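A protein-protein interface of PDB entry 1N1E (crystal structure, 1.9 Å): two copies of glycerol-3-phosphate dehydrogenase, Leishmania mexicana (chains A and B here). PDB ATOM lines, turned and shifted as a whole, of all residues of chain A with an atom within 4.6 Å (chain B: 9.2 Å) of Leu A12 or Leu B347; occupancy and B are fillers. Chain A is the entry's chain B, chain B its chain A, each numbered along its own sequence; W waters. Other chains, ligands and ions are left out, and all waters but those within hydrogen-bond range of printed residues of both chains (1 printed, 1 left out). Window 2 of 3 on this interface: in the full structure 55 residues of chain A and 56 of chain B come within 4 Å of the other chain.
O of Cys B345 touches OD1 of Asp A10, 3.98 Å away. CA of Gly B346 touches OD1 of Asp A10, 3.7 Å away. Leu A12 touches Leu B347. Gln A182 touches Leu B347 (NE2 to CB, 3.8 Å). CD2 of Leu B347 touches OG of Ser A186 (3.5 Å). CD2 of Leu B347 touches O of Cys A194 (3.8 Å).
O of Leu B343 sits at hydrogen-bond distance from NH2 of Arg A190 (3.2 Å). O of Gln B348 lies within hydrogen-bond range of NE2 of Gln A182 (2.7 Å). OD2 of Asp A10 sits close to O of Leu B347 (2.9 Å).
No position is printed for both chains. Of the 9 pairs that touch across the chains among the printed residues, none has its exchanged pair printed and touching as well.
Leu A12 touches just one residue of chain B: Leu B347 (3.8 Å). Of the printed residues of chain B, Gln A182 touches Leu B347 (3.8 Å) and Gln B348 (2.7 Å). Printed residues of chain A within 4 Å of Leu B343: Arg A190 (3.2 Å). Of the printed residues of chain A, Leu B347 touches Asp A10, Leu A12, Gln A182, Ser A186 and Cys A194.
The side-chain amino group (NZ) of Lys A37 sits at hydrogen-bond distance from the backbone carbonyl oxygen (O) of Ser A186 (2.8 Å). O of Gln A182 sits at hydrogen-bond distance from OG of Ser A186 (2.7 Å). The backbone carbonyl oxygen of Cys A194 is in hydrogen-bond range of the side-chain amide nitrogen of Gln A182, at 2.7 Å. OG of Ser A186 is in hydrogen-bond range of N of Cys A194.
Water W1 lies within hydrogen-bond range of the backbone carbonyl oxygen (O) of Cys A194 and the backbone NH (N) of Gln B348.
Hydrophobic or aromatic side chains of chain A that line the printed part of chain B: Leu A12. Of the 8 printed residues of chain B, 5 touch a printed residue of chain A.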
ATOM      1  N   ASP A  10     -18.709 -27.125  17.733  1.00  0.00           N
ATOM      2  CA  ASP A  10     -20.083 -26.665  17.928  1.00  0.00           C
ATOM      3  C   ASP A  10     -20.583 -25.850  16.715  1.00  0.00           C
ATOM      4  O   ASP A  10     -21.646 -25.221  16.785  1.00  0.00           O
ATOM      5  CB  ASP A  10     -20.181 -25.830  19.217  1.00  0.00           C
ATOM      6  CG  ASP A  10     -19.667 -26.580  20.459  1.00  0.00           C
ATOM      7  OD1 ASP A  10     -19.357 -25.910  21.474  1.00  0.00           O
ATOM      8  OD2 ASP A  10     -19.538 -27.827  20.518  1.00  0.00           O
ATOM      9  N   GLU A  11     -19.828 -25.875  15.609  1.00  0.00           N
ATOM     10  CA  GLU A  11     -20.185 -25.119  14.407  1.00  0.00           C
ATOM     11  C   GLU A  11     -20.918 -25.983  13.375  1.00  0.00           C
ATOM     12  O   GLU A  11     -20.555 -27.118  13.092  1.00  0.00           O
ATOM     13  CB  GLU A  11     -18.961 -24.449  13.769  1.00  0.00           C
ATOM     14  CG  GLU A  11     -19.146 -22.961  13.450  1.00  0.00           C
ATOM     15  CD  GLU A  11     -18.206 -22.052  14.243  1.00  0.00           C
ATOM     16  OE1 GLU A  11     -18.703 -21.141  14.947  1.00  0.00           O
ATOM     17  OE2 GLU A  11     -16.969 -22.243  14.163  1.00  0.00           O
ATOM     18  N   LEU A  12     -21.943 -25.393  12.797  1.00  0.00           N
ATOM     19  CA  LEU A  12     -22.898 -26.112  11.986  1.00  0.00           C
ATOM     20  C   LEU A  12     -22.337 -26.406  10.609  1.00  0.00           C
ATOM     21  O   LEU A  12     -21.474 -25.685  10.109  1.00  0.00           O
ATOM     22  CB  LEU A  12     -24.184 -25.305  11.882  1.00  0.00           C
ATOM     23  CG  LEU A  12     -24.791 -24.924  13.234  1.00  0.00           C
ATOM     24  CD1 LEU A  12     -26.076 -24.164  13.019  1.00  0.00           C
ATOM     25  CD2 LEU A  12     -25.019 -26.173  14.102  1.00  0.00           C
ATOM     26  N   LEU A  13     -22.824 -27.494  10.029  1.00  0.00           N
ATOM     27  CA  LEU A  13     -22.522 -27.876   8.664  1.00  0.00           C
ATOM     28  C   LEU A  13     -23.749 -27.659   7.803  1.00  0.00           C
ATOM     29  O   LEU A  13     -24.890 -27.774   8.270  1.00  0.00           O
ATOM     30  CB  LEU A  13     -22.074 -29.341   8.617  1.00  0.00           C
ATOM     31  CG  LEU A  13     -20.694 -29.598   9.236  1.00  0.00           C
ATOM     32  CD1 LEU A  13     -20.475 -31.074   9.463  1.00  0.00           C
ATOM     33  CD2 LEU A  13     -19.576 -29.020   8.346  1.00  0.00           C
ATOM     34  N   TYR A  14     -23.505 -27.334   6.540  1.00  0.00           N
ATOM     35  CA  TYR A  14     -24.547 -27.093   5.556  1.00  0.00           C
ATOM     36  C   TYR A  14     -24.280 -27.961   4.333  1.00  0.00           C
ATOM     37  O   TYR A  14     -23.133 -28.269   4.026  1.00  0.00           O
ATOM     38  CB  TYR A  14     -24.585 -25.599   5.180  1.00  0.00           C
ATOM     39  CG  TYR A  14     -24.680 -24.706   6.401  1.00  0.00           C
ATOM     40  CD1 TYR A  14     -23.544 -24.386   7.124  1.00  0.00           C
ATOM     41  CD2 TYR A  14     -25.900 -24.225   6.853  1.00  0.00           C
ATOM     42  CE1 TYR A  14     -23.609 -23.594   8.253  1.00  0.00           C
ATOM     43  CE2 TYR A  14     -25.975 -23.413   7.994  1.00  0.00           C
ATOM     44  CZ  TYR A  14     -24.810 -23.109   8.681  1.00  0.00           C
ATOM     45  OH  TYR A  14     -24.812 -22.327   9.817  1.00  0.00           O
ATOM     46  N   LYS A  37     -30.872 -25.997   6.352  1.00  0.00           N
ATOM     47  CA  LYS A  37     -29.482 -26.433   6.334  1.00  0.00           C
ATOM     48  C   LYS A  37     -28.944 -26.765   4.939  1.00  0.00           C
ATOM     49  O   LYS A  37     -27.738 -26.840   4.764  1.00  0.00           O
ATOM     50  CB  LYS A  37     -29.313 -27.647   7.256  1.00  0.00           C
ATOM     51  CG  LYS A  37     -29.727 -27.408   8.707  1.00  0.00           C
ATOM     52  CD  LYS A  37     -28.999 -26.252   9.380  1.00  0.00           C
ATOM     53  CE  LYS A  37     -27.472 -26.433   9.422  1.00  0.00           C
ATOM     54  NZ  LYS A  37     -26.978 -27.638  10.181  1.00  0.00           N
ATOM     55  N   GLN A 182     -24.985 -34.392  13.919  1.00  0.00           N
ATOM     56  CA  GLN A 182     -25.520 -33.431  14.853  1.00  0.00           C
ATOM     57  C   GLN A 182     -25.277 -32.008  14.318  1.00  0.00           C
ATOM     58  O   GLN A 182     -26.126 -31.141  14.454  1.00  0.00           O
ATOM     59  CB  GLN A 182     -24.903 -33.696  16.237  1.00  0.00           C
ATOM     60  CG  GLN A 182     -24.726 -32.529  17.158  1.00  0.00           C
ATOM     61  CD  GLN A 182     -24.009 -32.933  18.438  1.00  0.00           C
ATOM     62  OE1 GLN A 182     -22.868 -33.421  18.386  1.00  0.00           O
ATOM     63  NE2 GLN A 182     -24.661 -32.728  19.583  1.00  0.00           N
ATOM     64  N   ARG A 183     -24.134 -31.797  13.672  1.00  0.00           N
ATOM     65  CA  ARG A 183     -23.792 -30.505  13.080  1.00  0.00           C
ATOM     66  C   ARG A 183     -24.583 -30.225  11.802  1.00  0.00           C
ATOM     67  O   ARG A 183     -24.842 -29.072  11.481  1.00  0.00           O
ATOM     68  CB  ARG A 183     -22.288 -30.408  12.803  1.00  0.00           C
ATOM     69  CG  ARG A 183     -21.433 -30.341  14.069  1.00  0.00           C
ATOM     70  CD  ARG A 183     -19.965 -30.718  13.859  1.00  0.00           C
ATOM     71  NE  ARG A 183     -19.277 -29.714  13.050  1.00  0.00           N
ATOM     72  CZ  ARG A 183     -18.131 -29.900  12.390  1.00  0.00           C
ATOM     73  NH1 ARG A 183     -17.494 -31.066  12.428  1.00  0.00           N
ATOM     74  NH2 ARG A 183     -17.611 -28.892  11.695  1.00  0.00           N
ATOM     75  N   SER A 186     -28.674 -29.857  13.261  1.00  0.00           N
ATOM     76  CA  SER A 186     -28.965 -28.808  14.234  1.00  0.00           C
ATOM     77  C   SER A 186     -29.032 -27.439  13.545  1.00  0.00           C
ATOM     78  O   SER A 186     -28.311 -27.194  12.588  1.00  0.00           O
ATOM     79  CB  SER A 186     -27.925 -28.794  15.356  1.00  0.00           C
ATOM     80  OG  SER A 186     -27.966 -30.002  16.103  1.00  0.00           O
ATOM     81  N   THR A 187     -29.906 -26.567  14.027  1.00  0.00           N
ATOM     82  CA  THR A 187     -30.136 -25.285  13.364  1.00  0.00           C
ATOM     83  C   THR A 187     -29.571 -24.119  14.171  1.00  0.00           C
ATOM     84  O   THR A 187     -29.500 -24.162  15.389  1.00  0.00           O
ATOM     85  CB  THR A 187     -31.642 -25.078  13.052  1.00  0.00           C
ATOM     86  OG1 THR A 187     -32.428 -25.201  14.244  1.00  0.00           O
ATOM     87  CG2 THR A 187     -32.167 -26.197  12.134  1.00  0.00           C
ATOM     88  N   GLY A 188     -29.178 -23.064  13.464  1.00  0.00           N
ATOM     89  CA  GLY A 188     -28.510 -21.929  14.070  1.00  0.00           C
ATOM     90  C   GLY A 188     -29.467 -21.030  14.807  1.00  0.00           C
ATOM     91  O   GLY A 188     -29.052 -20.300  15.704  1.00  0.00           O
ATOM     92  N   ARG A 190     -31.449 -22.251  16.757  1.00  0.00           N
ATOM     93  CA  ARG A 190     -31.633 -23.080  17.949  1.00  0.00           C
ATOM     94  C   ARG A 190     -33.031 -23.687  18.077  1.00  0.00           C
ATOM     95  O   ARG A 190     -33.474 -23.994  19.174  1.00  0.00           O
ATOM     96  CB  ARG A 190     -31.266 -22.295  19.222  1.00  0.00           C
ATOM     97  CG  ARG A 190     -29.817 -21.749  19.258  1.00  0.00           C
ATOM     98  CD  ARG A 190     -28.693 -22.805  19.167  1.00  0.00           C
ATOM     99  NE  ARG A 190     -28.405 -23.438  20.463  1.00  0.00           N
ATOM    100  CZ  ARG A 190     -27.800 -24.624  20.627  1.00  0.00           C
ATOM    101  NH1 ARG A 190     -27.394 -25.342  19.578  1.00  0.00           N
ATOM    102  NH2 ARG A 190     -27.594 -25.099  21.858  1.00  0.00           N
ATOM    103  N   VAL A 193     -32.158 -29.005  18.039  1.00  0.00           N
ATOM    104  CA  VAL A 193     -30.874 -29.256  18.670  1.00  0.00           C
ATOM    105  C   VAL A 193     -30.676 -30.753  18.885  1.00  0.00           C
ATOM    106  O   VAL A 193     -31.491 -31.407  19.527  1.00  0.00           O
ATOM    107  CB  VAL A 193     -30.796 -28.547  20.020  1.00  0.00           C
ATOM    108  CG1 VAL A 193     -29.461 -28.839  20.713  1.00  0.00           C
ATOM    109  CG2 VAL A 193     -31.013 -27.052  19.823  1.00  0.00           C
ATOM    110  N   CYS A 194     -29.572 -31.266  18.360  1.00  0.00           N
ATOM    111  CA  CYS A 194     -29.250 -32.681  18.395  1.00  0.00           C
ATOM    112  C   CYS A 194     -28.164 -32.962  19.433  1.00  0.00           C
ATOM    113  O   CYS A 194     -27.274 -32.135  19.650  1.00  0.00           O
ATOM    114  CB  CYS A 194     -28.780 -33.126  17.013  1.00  0.00           C
ATOM    115  SG  CYS A 194     -30.060 -32.989  15.729  1.00  0.00           S
ATOM    116  N   LEU B 343     -29.294 -21.873  26.498  1.00  0.00           N
ATOM    117  CA  LEU B 343     -29.061 -22.416  25.147  1.00  0.00           C
ATOM    118  C   LEU B 343     -27.736 -21.991  24.506  1.00  0.00           C
ATOM    119  O   LEU B 343     -27.514 -22.263  23.325  1.00  0.00           O
ATOM    120  CB  LEU B 343     -30.208 -22.022  24.205  1.00  0.00           C
ATOM    121  CG  LEU B 343     -31.595 -22.581  24.523  1.00  0.00           C
ATOM    122  CD1 LEU B 343     -32.599 -22.141  23.462  1.00  0.00           C
ATOM    123  CD2 LEU B 343     -31.559 -24.094  24.648  1.00  0.00           C
ATOM    124  N   SER B 344     -26.852 -21.347  25.268  1.00  0.00           N
ATOM    125  CA  SER B 344     -25.584 -20.836  24.725  1.00  0.00           C
ATOM    126  C   SER B 344     -24.414 -21.827  24.866  1.00  0.00           C
ATOM    127  O   SER B 344     -23.263 -21.469  24.618  1.00  0.00           O
ATOM    128  CB  SER B 344     -25.224 -19.519  25.423  1.00  0.00           C
ATOM    129  OG  SER B 344     -24.958 -19.730  26.800  1.00  0.00           O
ATOM    130  N   CYS B 345     -24.709 -23.066  25.249  1.00  0.00           N
ATOM    131  CA  CYS B 345     -23.669 -24.044  25.570  1.00  0.00           C
ATOM    132  C   CYS B 345     -22.948 -24.652  24.353  1.00  0.00           C
ATOM    133  O   CYS B 345     -21.846 -25.187  24.493  1.00  0.00           O
ATOM    134  CB  CYS B 345     -24.253 -25.159  26.450  1.00  0.00           C
ATOM    135  SG  CYS B 345     -25.814 -25.854  25.842  1.00  0.00           S
ATOM    136  N   GLY B 346     -23.543 -24.573  23.165  1.00  0.00           N
ATOM    137  CA  GLY B 346     -22.973 -25.247  22.004  1.00  0.00           C
ATOM    138  C   GLY B 346     -23.315 -26.733  22.001  1.00  0.00           C
ATOM    139  O   GLY B 346     -23.843 -27.262  22.985  1.00  0.00           O
ATOM    140  N   LEU B 347     -23.012 -27.407  20.898  1.00  0.00           N
ATOM    141  CA  LEU B 347     -23.457 -28.787  20.690  1.00  0.00           C
ATOM    142  C   LEU B 347     -22.692 -29.769  21.580  1.00  0.00           C
ATOM    143  O   LEU B 347     -21.464 -29.704  21.675  1.00  0.00           O
ATOM    144  CB  LEU B 347     -23.326 -29.166  19.209  1.00  0.00           C
ATOM    145  CG  LEU B 347     -24.277 -28.406  18.274  1.00  0.00           C
ATOM    146  CD1 LEU B 347     -23.895 -28.592  16.816  1.00  0.00           C
ATOM    147  CD2 LEU B 347     -25.721 -28.828  18.509  1.00  0.00           C
ATOM    148  N   GLN B 348     -23.419 -30.671  22.239  1.00  0.00           N
ATOM    149  CA  GLN B 348     -22.793 -31.664  23.116  1.00  0.00           C
ATOM    150  C   GLN B 348     -23.284 -33.094  22.932  1.00  0.00           C
ATOM    151  O   GLN B 348     -24.247 -33.372  22.203  1.00  0.00           O
ATOM    152  CB  GLN B 348     -22.941 -31.291  24.600  1.00  0.00           C
ATOM    153  CG  GLN B 348     -23.792 -30.094  24.931  1.00  0.00           C
ATOM    154  CD  GLN B 348     -23.354 -29.454  26.223  1.00  0.00           C
ATOM    155  OE1 GLN B 348     -23.671 -29.952  27.305  1.00  0.00           O
ATOM    156  NE2 GLN B 348     -22.595 -28.362  26.120  1.00  0.00           N
ATOM    157  N   ASP B 349     -22.576 -34.002  23.594  1.00  0.00           N
ATOM    158  CA  ASP B 349     -23.029 -35.365  23.754  1.00  0.00           C
ATOM    159  C   ASP B 349     -24.178 -35.383  24.763  1.00  0.00           C
ATOM    160  O   ASP B 349     -24.276 -34.502  25.623  1.00  0.00           O
ATOM    161  CB  ASP B 349     -21.888 -36.245  24.255  1.00  0.00           C
ATOM    162  CG  ASP B 349     -20.790 -36.444  23.218  1.00  0.00           C
ATOM    163  OD1 ASP B 349     -20.895 -35.945  22.066  1.00  0.00           O
ATOM    164  OD2 ASP B 349     -19.780 -37.123  23.473  1.00  0.00           O
ATOM    165  N   GLU B 350     -25.038 -36.390  24.667  1.00  0.00           N
ATOM    166  CA  GLU B 350     -26.096 -36.568  25.651  1.00  0.00           C
ATOM    167  C   GLU B 350     -25.428 -36.800  27.004  1.00  0.00           C
ATOM    168  O   GLU B 350     -25.780 -36.172  28.000  1.00  0.00           O
ATOM    169  CB  GLU B 350     -27.012 -37.733  25.274  1.00  0.00           C
ATOM    170  CG  GLU B 350     -28.122 -37.974  26.291  1.00  0.00           C
ATOM    171  CD  GLU B 350     -29.381 -38.541  25.659  1.00  0.00           C
ATOM    172  OE1 GLU B 350     -29.403 -39.755  25.352  1.00  0.00           O
ATOM    173  OE2 GLU B 350     -30.335 -37.768  25.459  1.00  0.00           O
HETATM  174  O   HOH W   1     -26.415 -30.581  21.922  1.00  0.00           O
